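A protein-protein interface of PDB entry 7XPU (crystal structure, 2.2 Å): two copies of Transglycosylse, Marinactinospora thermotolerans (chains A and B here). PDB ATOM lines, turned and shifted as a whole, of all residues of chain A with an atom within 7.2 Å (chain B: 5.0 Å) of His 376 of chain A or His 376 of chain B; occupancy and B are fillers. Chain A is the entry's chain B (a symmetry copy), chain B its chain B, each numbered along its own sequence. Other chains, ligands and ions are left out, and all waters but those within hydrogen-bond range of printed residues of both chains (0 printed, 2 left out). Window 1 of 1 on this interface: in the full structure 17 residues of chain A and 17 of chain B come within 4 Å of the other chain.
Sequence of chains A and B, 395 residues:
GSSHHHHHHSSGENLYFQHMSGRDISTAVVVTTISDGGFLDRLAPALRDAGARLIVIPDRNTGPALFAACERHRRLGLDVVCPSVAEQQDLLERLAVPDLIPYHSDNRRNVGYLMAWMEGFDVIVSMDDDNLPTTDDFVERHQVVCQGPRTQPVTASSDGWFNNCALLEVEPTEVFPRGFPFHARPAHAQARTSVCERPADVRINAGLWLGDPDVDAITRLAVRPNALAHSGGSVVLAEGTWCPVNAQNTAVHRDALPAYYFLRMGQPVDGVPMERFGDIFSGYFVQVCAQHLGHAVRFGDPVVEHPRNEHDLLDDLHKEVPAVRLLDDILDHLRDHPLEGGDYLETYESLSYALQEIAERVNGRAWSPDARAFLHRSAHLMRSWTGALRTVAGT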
ATOM      1  N   GLN A 267      12.199  25.605 -10.088  1.00  0.00           N
ATOM      2  CA  GLN A 267      10.913  25.535 -10.771  1.00  0.00           C
ATOM      3  C   GLN A 267       9.788  25.420  -9.747  1.00  0.00           C
ATOM      4  O   GLN A 267       9.854  24.569  -8.852  1.00  0.00           O
ATOM      5  CB  GLN A 267      10.874  24.350 -11.734  1.00  0.00           C
ATOM      6  CG  GLN A 267      11.819  24.477 -12.923  1.00  0.00           C
ATOM      7  CD  GLN A 267      11.423  25.590 -13.877  1.00  0.00           C
ATOM      8  OE1 GLN A 267      12.269  26.166 -14.559  1.00  0.00           O
ATOM      9  NE2 GLN A 267      10.129  25.892 -13.937  1.00  0.00           N
ATOM     10  N   SER A 352      15.361  12.225 -21.512  1.00  0.00           N
ATOM     11  CA  SER A 352      14.784  13.566 -21.511  1.00  0.00           C
ATOM     12  C   SER A 352      13.452  13.598 -22.250  1.00  0.00           C
ATOM     13  O   SER A 352      12.496  14.234 -21.791  1.00  0.00           O
ATOM     14  CB  SER A 352      15.766  14.558 -22.133  1.00  0.00           C
ATOM     15  OG  SER A 352      15.967  14.273 -23.507  1.00  0.00           O
ATOM     16  N   TYR A 353      13.369  12.923 -23.400  1.00  0.00           N
ATOM     17  CA  TYR A 353      12.096  12.846 -24.109  1.00  0.00           C
ATOM     18  C   TYR A 353      11.072  12.034 -23.328  1.00  0.00           C
ATOM     19  O   TYR A 353       9.872  12.318 -23.400  1.00  0.00           O
ATOM     20  CB  TYR A 353      12.291  12.247 -25.502  1.00  0.00           C
ATOM     21  CG  TYR A 353      13.281  12.990 -26.370  1.00  0.00           C
ATOM     22  CD1 TYR A 353      13.033  14.294 -26.783  1.00  0.00           C
ATOM     23  CD2 TYR A 353      14.455  12.382 -26.793  1.00  0.00           C
ATOM     24  CE1 TYR A 353      13.936  14.974 -27.583  1.00  0.00           C
ATOM     25  CE2 TYR A 353      15.362  13.053 -27.590  1.00  0.00           C
ATOM     26  CZ  TYR A 353      15.098  14.347 -27.983  1.00  0.00           C
ATOM     27  OH  TYR A 353      16.001  15.014 -28.778  1.00  0.00           O
ATOM     28  N   LEU A 355      10.774  11.968 -20.060  1.00  0.00           N
ATOM     29  CA  LEU A 355      10.236  12.838 -19.019  1.00  0.00           C
ATOM     30  C   LEU A 355       9.143  13.750 -19.560  1.00  0.00           C
ATOM     31  O   LEU A 355       8.220  14.117 -18.823  1.00  0.00           O
ATOM     32  CB  LEU A 355      11.357  13.670 -18.394  1.00  0.00           C
ATOM     33  CG  LEU A 355      12.466  12.908 -17.664  1.00  0.00           C
ATOM     34  CD1 LEU A 355      13.540  13.867 -17.183  1.00  0.00           C
ATOM     35  CD2 LEU A 355      11.897  12.119 -16.500  1.00  0.00           C
ATOM     36  N   GLN A 356       9.224  14.125 -20.840  1.00  0.00           N
ATOM     37  CA  GLN A 356       8.196  14.978 -21.425  1.00  0.00           C
ATOM     38  C   GLN A 356       6.903  14.208 -21.657  1.00  0.00           C
ATOM     39  O   GLN A 356       5.809  14.765 -21.513  1.00  0.00           O
ATOM     40  CB  GLN A 356       8.702  15.588 -22.730  1.00  0.00           C
ATOM     41  CG  GLN A 356       9.938  16.446 -22.558  1.00  0.00           C
ATOM     42  CD  GLN A 356      10.299  17.201 -23.815  1.00  0.00           C
ATOM     43  OE1 GLN A 356      11.105  16.738 -24.620  1.00  0.00           O
ATOM     44  NE2 GLN A 356       9.703  18.377 -23.991  1.00  0.00           N
ATOM     45  N   GLU A 357       7.007  12.930 -22.030  1.00  0.00           N
ATOM     46  CA  GLU A 357       5.813  12.102 -22.149  1.00  0.00           C
ATOM     47  C   GLU A 357       5.179  11.863 -20.786  1.00  0.00           C
ATOM     48  O   GLU A 357       3.949  11.849 -20.658  1.00  0.00           O
ATOM     49  CB  GLU A 357       6.160  10.771 -22.818  1.00  0.00           C
ATOM     50  CG  GLU A 357       6.938  10.909 -24.118  1.00  0.00           C
ATOM     51  CD  GLU A 357       6.131  11.570 -25.219  1.00  0.00           C
ATOM     52  OE1 GLU A 357       4.896  11.387 -25.247  1.00  0.00           O
ATOM     53  OE2 GLU A 357       6.733  12.276 -26.056  1.00  0.00           O
ATOM     54  N   ILE A 358       6.006  11.687 -19.754  1.00  0.00           N
ATOM     55  CA  ILE A 358       5.491  11.469 -18.406  1.00  0.00           C
ATOM     56  C   ILE A 358       4.779  12.716 -17.897  1.00  0.00           C
ATOM     57  O   ILE A 358       3.752  12.624 -17.214  1.00  0.00           O
ATOM     58  CB  ILE A 358       6.640  11.043 -17.474  1.00  0.00           C
ATOM     59  CG1 ILE A 358       7.174   9.671 -17.886  1.00  0.00           C
ATOM     60  CG2 ILE A 358       6.189  11.041 -16.020  1.00  0.00           C
ATOM     61  CD1 ILE A 358       8.447   9.270 -17.180  1.00  0.00           C
ATOM     62  N   ALA A 359       5.297  13.899 -18.238  1.00  0.00           N
ATOM     63  CA  ALA A 359       4.718  15.147 -17.752  1.00  0.00           C
ATOM     64  C   ALA A 359       3.275  15.342 -18.198  1.00  0.00           C
ATOM     65  O   ALA A 359       2.533  16.085 -17.546  1.00  0.00           O
ATOM     66  CB  ALA A 359       5.566  16.333 -18.214  1.00  0.00           C
ATOM     67  N   GLU A 360       2.855  14.696 -19.286  1.00  0.00           N
ATOM     68  CA  GLU A 360       1.499  14.853 -19.793  1.00  0.00           C
ATOM     69  C   GLU A 360       0.576  13.700 -19.429  1.00  0.00           C
ATOM     70  O   GLU A 360      -0.647  13.882 -19.436  1.00  0.00           O
ATOM     71  CB  GLU A 360       1.518  15.021 -21.318  1.00  0.00           C
ATOM     72  CG  GLU A 360       2.335  16.212 -21.797  1.00  0.00           C
ATOM     73  CD  GLU A 360       1.857  17.526 -21.206  1.00  0.00           C
ATOM     74  OE1 GLU A 360       0.627  17.724 -21.100  1.00  0.00           O
ATOM     75  OE2 GLU A 360       2.711  18.360 -20.839  1.00  0.00           O
ATOM     76  N   PRO A 369      -0.168  23.085 -13.896  1.00  0.00           N
ATOM     77  CA  PRO A 369       0.570  23.399 -15.135  1.00  0.00           C
ATOM     78  C   PRO A 369       2.041  23.729 -14.922  1.00  0.00           C
ATOM     79  O   PRO A 369       2.873  23.353 -15.757  1.00  0.00           O
ATOM     80  CB  PRO A 369      -0.208  24.594 -15.699  1.00  0.00           C
ATOM     81  CG  PRO A 369      -1.601  24.369 -15.232  1.00  0.00           C
ATOM     82  CD  PRO A 369      -1.481  23.762 -13.858  1.00  0.00           C
ATOM     83  N   ALA A 371       3.926  22.495 -12.562  1.00  0.00           N
ATOM     84  CA  ALA A 371       4.608  21.255 -12.204  1.00  0.00           C
ATOM     85  C   ALA A 371       4.915  20.422 -13.442  1.00  0.00           C
ATOM     86  O   ALA A 371       6.013  19.867 -13.568  1.00  0.00           O
ATOM     87  CB  ALA A 371       3.764  20.458 -11.209  1.00  0.00           C
ATOM     88  N   ARG A 372       3.958  20.327 -14.369  1.00  0.00           N
ATOM     89  CA  ARG A 372       4.202  19.600 -15.610  1.00  0.00           C
ATOM     90  C   ARG A 372       5.277  20.283 -16.448  1.00  0.00           C
ATOM     91  O   ARG A 372       6.144  19.613 -17.020  1.00  0.00           O
ATOM     92  CB  ARG A 372       2.903  19.467 -16.405  1.00  0.00           C
ATOM     93  CG  ARG A 372       1.781  18.761 -15.657  1.00  0.00           C
ATOM     94  CD  ARG A 372       0.531  18.649 -16.517  1.00  0.00           C
ATOM     95  NE  ARG A 372      -0.572  18.013 -15.805  1.00  0.00           N
ATOM     96  CZ  ARG A 372      -0.792  16.706 -15.774  1.00  0.00           C
ATOM     97  NH1 ARG A 372       0.003  15.857 -16.406  1.00  0.00           N
ATOM     98  NH2 ARG A 372      -1.833  16.238 -15.093  1.00  0.00           N
ATOM     99  N   ALA A 373       5.241  21.616 -16.524  1.00  0.00           N
ATOM    100  CA  ALA A 373       6.240  22.346 -17.295  1.00  0.00           C
ATOM    101  C   ALA A 373       7.631  22.249 -16.682  1.00  0.00           C
ATOM    102  O   ALA A 373       8.621  22.504 -17.379  1.00  0.00           O
ATOM    103  CB  ALA A 373       5.829  23.812 -17.436  1.00  0.00           C
ATOM    104  N   PHE A 374       7.730  21.893 -15.399  1.00  0.00           N
ATOM    105  CA  PHE A 374       9.037  21.661 -14.795  1.00  0.00           C
ATOM    106  C   PHE A 374       9.771  20.517 -15.487  1.00  0.00           C
ATOM    107  O   PHE A 374      10.976  20.609 -15.745  1.00  0.00           O
ATOM    108  CB  PHE A 374       8.878  21.385 -13.298  1.00  0.00           C
ATOM    109  CG  PHE A 374       9.893  20.426 -12.743  1.00  0.00           C
ATOM    110  CD1 PHE A 374      11.205  20.821 -12.535  1.00  0.00           C
ATOM    111  CD2 PHE A 374       9.529  19.130 -12.413  1.00  0.00           C
ATOM    112  CE1 PHE A 374      12.137  19.938 -12.022  1.00  0.00           C
ATOM    113  CE2 PHE A 374      10.455  18.243 -11.899  1.00  0.00           C
ATOM    114  CZ  PHE A 374      11.760  18.648 -11.703  1.00  0.00           C
ATOM    115  N   LEU A 375       9.059  19.434 -15.806  1.00  0.00           N
ATOM    116  CA  LEU A 375       9.699  18.313 -16.491  1.00  0.00           C
ATOM    117  C   LEU A 375      10.084  18.672 -17.921  1.00  0.00           C
ATOM    118  O   LEU A 375      11.020  18.082 -18.474  1.00  0.00           O
ATOM    119  CB  LEU A 375       8.782  17.091 -16.477  1.00  0.00           C
ATOM    120  CG  LEU A 375       8.582  16.405 -15.122  1.00  0.00           C
ATOM    121  CD1 LEU A 375       7.538  15.302 -15.210  1.00  0.00           C
ATOM    122  CD2 LEU A 375       9.900  15.849 -14.610  1.00  0.00           C
ATOM    123  N   HIS A 376       9.388  19.632 -18.533  1.00  0.00           N
ATOM    124  CA  HIS A 376       9.703  20.012 -19.906  1.00  0.00           C
ATOM    125  C   HIS A 376      10.943  20.896 -19.968  1.00  0.00           C
ATOM    126  O   HIS A 376      11.826  20.680 -20.806  1.00  0.00           O
ATOM    127  CB  HIS A 376       8.506  20.715 -20.548  1.00  0.00           C
ATOM    128  CG  HIS A 376       7.339  19.812 -20.794  1.00  0.00           C
ATOM    129  ND1 HIS A 376       7.319  18.883 -21.813  1.00  0.00           N
ATOM    130  CD2 HIS A 376       6.152  19.693 -20.153  1.00  0.00           C
ATOM    131  CE1 HIS A 376       6.169  18.232 -21.788  1.00  0.00           C
ATOM    132  NE2 HIS A 376       5.444  18.704 -20.792  1.00  0.00           N
ATOM    133  N   ARG A 377      11.028  21.901 -19.093  1.00  0.00           N
ATOM    134  CA  ARG A 377      12.218  22.747 -19.074  1.00  0.00           C
ATOM    135  C   ARG A 377      13.438  21.965 -18.606  1.00  0.00           C
ATOM    136  O   ARG A 377      14.544  22.163 -19.122  1.00  0.00           O
ATOM    137  CB  ARG A 377      11.986  23.973 -18.191  1.00  0.00           C
ATOM    138  CG  ARG A 377      13.202  24.884 -18.080  1.00  0.00           C
ATOM    139  CD  ARG A 377      12.807  26.317 -17.760  1.00  0.00           C
ATOM    140  NE  ARG A 377      13.950  27.220 -17.825  1.00  0.00           N
ATOM    141  CZ  ARG A 377      14.518  27.794 -16.773  1.00  0.00           C
ATOM    142  NH1 ARG A 377      14.055  27.610 -15.547  1.00  0.00           N
ATOM    143  NH2 ARG A 377      15.576  28.581 -16.956  1.00  0.00           N
ATOM    144  N   SER A 378      13.253  21.066 -17.635  1.00  0.00           N
ATOM    145  CA  SER A 378      14.353  20.211 -17.200  1.00  0.00           C
ATOM    146  C   SER A 378      14.860  19.344 -18.345  1.00  0.00           C
ATOM    147  O   SER A 378      16.069  19.121 -18.477  1.00  0.00           O
ATOM    148  CB  SER A 378      13.911  19.336 -16.028  1.00  0.00           C
ATOM    149  OG  SER A 378      13.480  20.123 -14.933  1.00  0.00           O
ATOM    150  N   ALA A 379      13.947  18.850 -19.186  1.00  0.00           N
ATOM    151  CA  ALA A 379      14.348  18.007 -20.306  1.00  0.00           C
ATOM    152  C   ALA A 379      15.180  18.786 -21.314  1.00  0.00           C
ATOM    153  O   ALA A 379      16.173  18.270 -21.840  1.00  0.00           O
ATOM    154  CB  ALA A 379      13.111  17.408 -20.977  1.00  0.00           C
ATOM    155  N   HIS A 380      14.789  20.032 -21.599  1.00  0.00           N
ATOM    156  CA  HIS A 380      15.576  20.864 -22.503  1.00  0.00           C
ATOM    157  C   HIS A 380      16.957  21.150 -21.928  1.00  0.00           C
ATOM    158  O   HIS A 380      17.951  21.168 -22.662  1.00  0.00           O
ATOM    159  CB  HIS A 380      14.841  22.171 -22.792  1.00  0.00           C
ATOM    160  CG  HIS A 380      15.653  23.155 -23.573  1.00  0.00           C
ATOM    161  ND1 HIS A 380      15.740  23.122 -24.949  1.00  0.00           N
ATOM    162  CD2 HIS A 380      16.424  24.194 -23.172  1.00  0.00           C
ATOM    163  CE1 HIS A 380      16.523  24.103 -25.361  1.00  0.00           C
ATOM    164  NE2 HIS A 380      16.951  24.768 -24.302  1.00  0.00           N
ATOM    165  N   LEU A 381      17.037  21.387 -20.616  1.00  0.00           N
ATOM    166  CA  LEU A 381      18.330  21.658 -19.998  1.00  0.00           C
ATOM    167  C   LEU A 381      19.208  20.416 -19.979  1.00  0.00           C
ATOM    168  O   LEU A 381      20.437  20.526 -20.058  1.00  0.00           O
ATOM    169  CB  LEU A 381      18.135  22.199 -18.580  1.00  0.00           C
ATOM    170  CG  LEU A 381      17.432  23.552 -18.449  1.00  0.00           C
ATOM    171  CD1 LEU A 381      17.320  23.964 -16.986  1.00  0.00           C
ATOM    172  CD2 LEU A 381      18.160  24.617 -19.253  1.00  0.00           C
ATOM    173  N   MET A 382      18.601  19.232 -19.872  1.00  0.00           N
ATOM    174  CA  MET A 382      19.368  17.997 -19.978  1.00  0.00           C
ATOM    175  C   MET A 382      19.985  17.855 -21.363  1.00  0.00           C
ATOM    176  O   MET A 382      21.163  17.500 -21.493  1.00  0.00           O
ATOM    177  CB  MET A 382      18.474  16.798 -19.657  1.00  0.00           C
ATOM    178  CG  MET A 382      18.059  16.706 -18.196  1.00  0.00           C
ATOM    179  SD  MET A 382      16.658  15.599 -17.942  1.00  0.00           S
ATOM    180  CE  MET A 382      17.291  14.089 -18.669  1.00  0.00           C
ATOM    181  N   ARG A 383      19.206  18.138 -22.413  1.00  0.00           N
ATOM    182  CA  ARG A 383      19.738  18.061 -23.771  1.00  0.00           C
ATOM    183  C   ARG A 383      20.701  19.205 -24.061  1.00  0.00           C
ATOM    184  O   ARG A 383      21.570  19.074 -24.931  1.00  0.00           O
ATOM    185  CB  ARG A 383      18.595  18.055 -24.786  1.00  0.00           C
ATOM    186  CG  ARG A 383      17.704  16.825 -24.698  1.00  0.00           C
ATOM    187  CD  ARG A 383      16.710  16.765 -25.855  1.00  0.00           C
ATOM    188  NE  ARG A 383      15.737  17.849 -25.797  1.00  0.00           N
ATOM    189  CZ  ARG A 383      14.590  17.791 -25.135  1.00  0.00           C
ATOM    190  NH1 ARG A 383      14.236  16.711 -24.459  1.00  0.00           N
ATOM    191  NH2 ARG A 383      13.780  18.846 -25.147  1.00  0.00           N
ATOM    192  N   GLN B 356      12.258  27.076 -27.510  1.00  0.00           N
ATOM    193  CA  GLN B 356      12.994  26.587 -26.349  1.00  0.00           C
ATOM    194  C   GLN B 356      14.326  27.309 -26.193  1.00  0.00           C
ATOM    195  O   GLN B 356      14.774  27.557 -25.068  1.00  0.00           O
ATOM    196  CB  GLN B 356      13.207  25.079 -26.459  1.00  0.00           C
ATOM    197  CG  GLN B 356      11.917  24.289 -26.525  1.00  0.00           C
ATOM    198  CD  GLN B 356      12.145  22.799 -26.427  1.00  0.00           C
ATOM    199  OE1 GLN B 356      12.263  22.110 -27.439  1.00  0.00           O
ATOM    200  NE2 GLN B 356      12.207  22.290 -25.200  1.00  0.00           N
ATOM    201  N   ALA B 359      13.458  30.703 -24.746  1.00  0.00           N
ATOM    202  CA  ALA B 359      13.075  30.656 -23.339  1.00  0.00           C
ATOM    203  C   ALA B 359      14.267  30.775 -22.398  1.00  0.00           C
ATOM    204  O   ALA B 359      14.090  31.178 -21.243  1.00  0.00           O
ATOM    205  CB  ALA B 359      12.314  29.362 -23.047  1.00  0.00           C
ATOM    206  N   GLU B 360      15.473  30.440 -22.857  1.00  0.00           N
ATOM    207  CA  GLU B 360      16.656  30.498 -22.010  1.00  0.00           C
ATOM    208  C   GLU B 360      17.517  31.730 -22.252  1.00  0.00           C
ATOM    209  O   GLU B 360      18.293  32.105 -21.366  1.00  0.00           O
ATOM    210  CB  GLU B 360      17.512  29.240 -22.205  1.00  0.00           C
ATOM    211  CG  GLU B 360      16.779  27.943 -21.894  1.00  0.00           C
ATOM    212  CD  GLU B 360      16.237  27.902 -20.476  1.00  0.00           C
ATOM    213  OE1 GLU B 360      16.943  28.358 -19.551  1.00  0.00           O
ATOM    214  OE2 GLU B 360      15.100  27.421 -20.288  1.00  0.00           O
ATOM    215  N   ARG B 372       9.517  30.864 -18.225  1.00  0.00           N
ATOM    216  CA  ARG B 372      10.391  30.196 -19.184  1.00  0.00           C
ATOM    217  C   ARG B 372       9.898  28.787 -19.492  1.00  0.00           C
ATOM    218  O   ARG B 372       9.911  28.358 -20.651  1.00  0.00           O
ATOM    219  CB  ARG B 372      11.824  30.162 -18.653  1.00  0.00           C
ATOM    220  CG  ARG B 372      12.413  31.533 -18.353  1.00  0.00           C
ATOM    221  CD  ARG B 372      13.844  31.419 -17.848  1.00  0.00           C
ATOM    222  NE  ARG B 372      14.414  32.719 -17.513  1.00  0.00           N
ATOM    223  CZ  ARG B 372      15.054  33.502 -18.371  1.00  0.00           C
ATOM    224  NH1 ARG B 372      15.224  33.148 -19.635  1.00  0.00           N
ATOM    225  NH2 ARG B 372      15.537  34.668 -17.951  1.00  0.00           N
ATOM    226  N   ALA B 373       9.452  28.056 -18.467  1.00  0.00           N
ATOM    227  CA  ALA B 373       8.953  26.702 -18.679  1.00  0.00           C
ATOM    228  C   ALA B 373       7.656  26.680 -19.479  1.00  0.00           C
ATOM    229  O   ALA B 373       7.303  25.632 -20.033  1.00  0.00           O
ATOM    230  CB  ALA B 373       8.752  25.998 -17.337  1.00  0.00           C
ATOM    231  N   PHE B 374       6.941  27.806 -19.549  1.00  0.00           N
ATOM    232  CA  PHE B 374       5.760  27.879 -20.403  1.00  0.00           C
ATOM    233  C   PHE B 374       6.123  27.656 -21.868  1.00  0.00           C
ATOM    234  O   PHE B 374       5.415  26.943 -22.588  1.00  0.00           O
ATOM    235  CB  PHE B 374       5.061  29.226 -20.210  1.00  0.00           C
ATOM    236  CG  PHE B 374       4.395  29.751 -21.450  1.00  0.00           C
ATOM    237  CD1 PHE B 374       3.210  29.196 -21.909  1.00  0.00           C
ATOM    238  CD2 PHE B 374       4.947  30.812 -22.151  1.00  0.00           C
ATOM    239  CE1 PHE B 374       2.597  29.682 -23.049  1.00  0.00           C
ATOM    240  CE2 PHE B 374       4.338  31.303 -23.289  1.00  0.00           C
ATOM    241  CZ  PHE B 374       3.162  30.737 -23.739  1.00  0.00           C
ATOM    242  N   LEU B 375       7.230  28.247 -22.325  1.00  0.00           N
ATOM    243  CA  LEU B 375       7.643  28.053 -23.712  1.00  0.00           C
ATOM    244  C   LEU B 375       8.114  26.626 -23.966  1.00  0.00           C
ATOM    245  O   LEU B 375       8.037  26.145 -25.103  1.00  0.00           O
ATOM    246  CB  LEU B 375       8.741  29.050 -24.081  1.00  0.00           C
ATOM    247  CG  LEU B 375       8.314  30.516 -24.206  1.00  0.00           C
ATOM    248  CD1 LEU B 375       9.517  31.423 -24.428  1.00  0.00           C
ATOM    249  CD2 LEU B 375       7.310  30.683 -25.332  1.00  0.00           C
ATOM    250  N   HIS B 376       8.596  25.934 -22.932  1.00  0.00           N
ATOM    251  CA  HIS B 376       9.071  24.567 -23.115  1.00  0.00           C
ATOM    252  C   HIS B 376       7.912  23.582 -23.212  1.00  0.00           C
ATOM    253  O   HIS B 376       7.901  22.711 -24.089  1.00  0.00           O
ATOM    254  CB  HIS B 376      10.016  24.179 -21.977  1.00  0.00           C
ATOM    255  CG  HIS B 376      11.321  24.910 -22.003  1.00  0.00           C
ATOM    256  ND1 HIS B 376      12.319  24.618 -22.908  1.00  0.00           N
ATOM    257  CD2 HIS B 376      11.793  25.922 -21.236  1.00  0.00           C
ATOM    258  CE1 HIS B 376      13.349  25.419 -22.697  1.00  0.00           C
ATOM    259  NE2 HIS B 376      13.055  26.219 -21.688  1.00  0.00           N
ATOM    260  N   ARG B 377       6.927  23.699 -22.317  1.00  0.00           N
ATOM    261  CA  ARG B 377       5.768  22.816 -22.396  1.00  0.00           C
ATOM    262  C   ARG B 377       4.945  23.103 -23.644  1.00  0.00           C
ATOM    263  O   ARG B 377       4.422  22.177 -24.276  1.00  0.00           O
ATOM    264  CB  ARG B 377       4.911  22.949 -21.137  1.00  0.00           C
ATOM    265  CG  ARG B 377       3.652  22.092 -21.162  1.00  0.00           C
ATOM    266  CD  ARG B 377       3.172  21.750 -19.761  1.00  0.00           C
ATOM    267  NE  ARG B 377       2.073  20.791 -19.785  1.00  0.00           N
ATOM    268  CZ  ARG B 377       0.815  21.078 -19.478  1.00  0.00           C
ATOM    269  NH1 ARG B 377       0.456  22.289 -19.085  1.00  0.00           N
ATOM    270  NH2 ARG B 377      -0.107  20.122 -19.562  1.00  0.00           N
ATOM    271  N   SER B 378       4.827  24.380 -24.019  1.00  0.00           N
ATOM    272  CA  SER B 378       4.134  24.726 -25.257  1.00  0.00           C
ATOM    273  C   SER B 378       4.822  24.102 -26.463  1.00  0.00           C
ATOM    274  O   SER B 378       4.157  23.647 -27.401  1.00  0.00           O
ATOM    275  CB  SER B 378       4.061  26.244 -25.415  1.00  0.00           C
ATOM    276  OG  SER B 378       3.382  26.842 -24.326  1.00  0.00           O
ATOM    277  N   ALA B 379       6.158  24.069 -26.454  1.00  0.00           N
ATOM    278  CA  ALA B 379       6.895  23.492 -27.572  1.00  0.00           C
ATOM    279  C   ALA B 379       6.637  21.997 -27.692  1.00  0.00           C
ATOM    280  O   ALA B 379       6.475  21.476 -28.802  1.00  0.00           O
ATOM    281  CB  ALA B 379       8.390  23.769 -27.410  1.00  0.00           C
ATOM    282  N   HIS B 380       6.597  21.289 -26.560  1.00  0.00           N
ATOM    283  CA  HIS B 380       6.285  19.864 -26.592  1.00  0.00           C
ATOM    284  C   HIS B 380       4.870  19.620 -27.101  1.00  0.00           C
ATOM    285  O   HIS B 380       4.628  18.664 -27.845  1.00  0.00           O
ATOM    286  CB  HIS B 380       6.461  19.255 -25.202  1.00  0.00           C
ATOM    287  CG  HIS B 380       5.998  17.835 -25.107  1.00  0.00           C
ATOM    288  ND1 HIS B 380       6.792  16.768 -25.467  1.00  0.00           N
ATOM    289  CD2 HIS B 380       4.818  17.307 -24.704  1.00  0.00           C
ATOM    290  CE1 HIS B 380       6.125  15.643 -25.281  1.00  0.00           C
ATOM    291  NE2 HIS B 380       4.924  15.943 -24.819  1.00  0.00           N
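The side-chain carboxylate of Glu 360 of chain B is in salt-bridge range of the guanidinium group of Arg 377 of chain A (2.7 Å). The side-chain carboxylate (OE2) of Glu 360 of chain A lies within salt-bridge range of the guanidinium group (NE) of Arg 377 of chain B, 2.7 Å away.
Hydrophobic or aromatic side chains of chain A that line the printed part of chain B: Ala 373, His 376, His 380 and Leu 381. Of the 12 printed residues of chain B, 7 touch a printed residue of chain A. Printed residues of chain B that touch a printed residue of chain A: Gln 356, Glu 360, Arg 372, Ala 373, His 376, Arg 377 and His 380. Among the printed residues, 20 pairs touch across the chains. Among the printed residues, Asp or Glu carboxylates within 4 Å of a Lys or Arg side-chain nitrogen of the other chain: Glu 360 of chain A with Arg 377 of chain B (2.7 Å) and Arg 377 of chain A with Glu 360 of chain B (2.7 Å).
A ring nitrogen (ND1) of His 376 of chain B sits at hydrogen-bond distance from the side-chain amide nitrogen (NE2) of Gln 356 of chain B. The guanidinium group (NH1) of Arg 383 of chain A is in hydrogen-bond range of the side-chain hydroxyl (OG) of Ser 352 of chain A (3.1 Å). NE2 of Gln 356 of chain A is in hydrogen-bond range of ND1 of His 376 of chain A, at 3.3 Å. NH1 of Arg 383 of chain A lies within hydrogen-bond range of OE1 of Gln 356 of chain A. NH1 of Arg 372 of chain A sits at hydrogen-bond distance from O of Ala 359 of chain A (2.8 Å). The side-chain carboxylate of Glu 360 of chain A sits at hydrogen-bond distance from a ring nitrogen (NE2) of His 376 of chain A (2.8 Å).
Gln 356 of chain A touches His 380 of chain B. His 380 of chain B touches Glu 360 of chain A (CD2 to CG, 3.98 Å). Arg 372 of chain A touches Arg 377 of chain B (CD to NH2, 3.4 Å). O of Ala 373 of chain A touches CB of Ala 373 of chain B, at 3.5 Å. Ala 373 of chain A touches Arg 377 of chain B. CD2 of His 380 of chain B touches CE1 of His 376 of chain A, at 3.3 Å. Arg 377 of chain A touches Arg 372 of chain B (NH2 to CD, 3.4 Å). CG of Arg 377 of chain A touches CD2 of His 376 of chain B (3.6 Å). His 380 of chain A touches Glu 360 of chain B (CD2 to CG, 3.98 Å). Arg 383 of chain A touches Gln 356 of chain B.
His 376 of chain A touches three residues of chain B. His 376 of chain B touches three residues of chain A. Printed residues of chain B within 4 Å of Glu 360 of chain A: Arg 377 and His 380. Printed residues of chain B within 4 Å of Gln 356 of chain A: His 380. Leu 375 of chain B touches none of the printed residues of chain A.
Gln 356 of chain A touches His 380 of chain B, and with the chains exchanged His 380 of chain A touches Gln 356 of chain B. Glu 360 of chain A touches Arg 377 of chain B, and with the chains exchanged Arg 377 of chain A touches Glu 360 of chain B. Arg 372 of chain A touches Arg 377 of chain B, and with the chains exchanged Arg 377 of chain A touches Arg 372 of chain B. Ala 373 of chain A touches Arg 377 of chain B, and with the chains exchanged Arg 377 of chain A touches Ala 373 of chain B.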
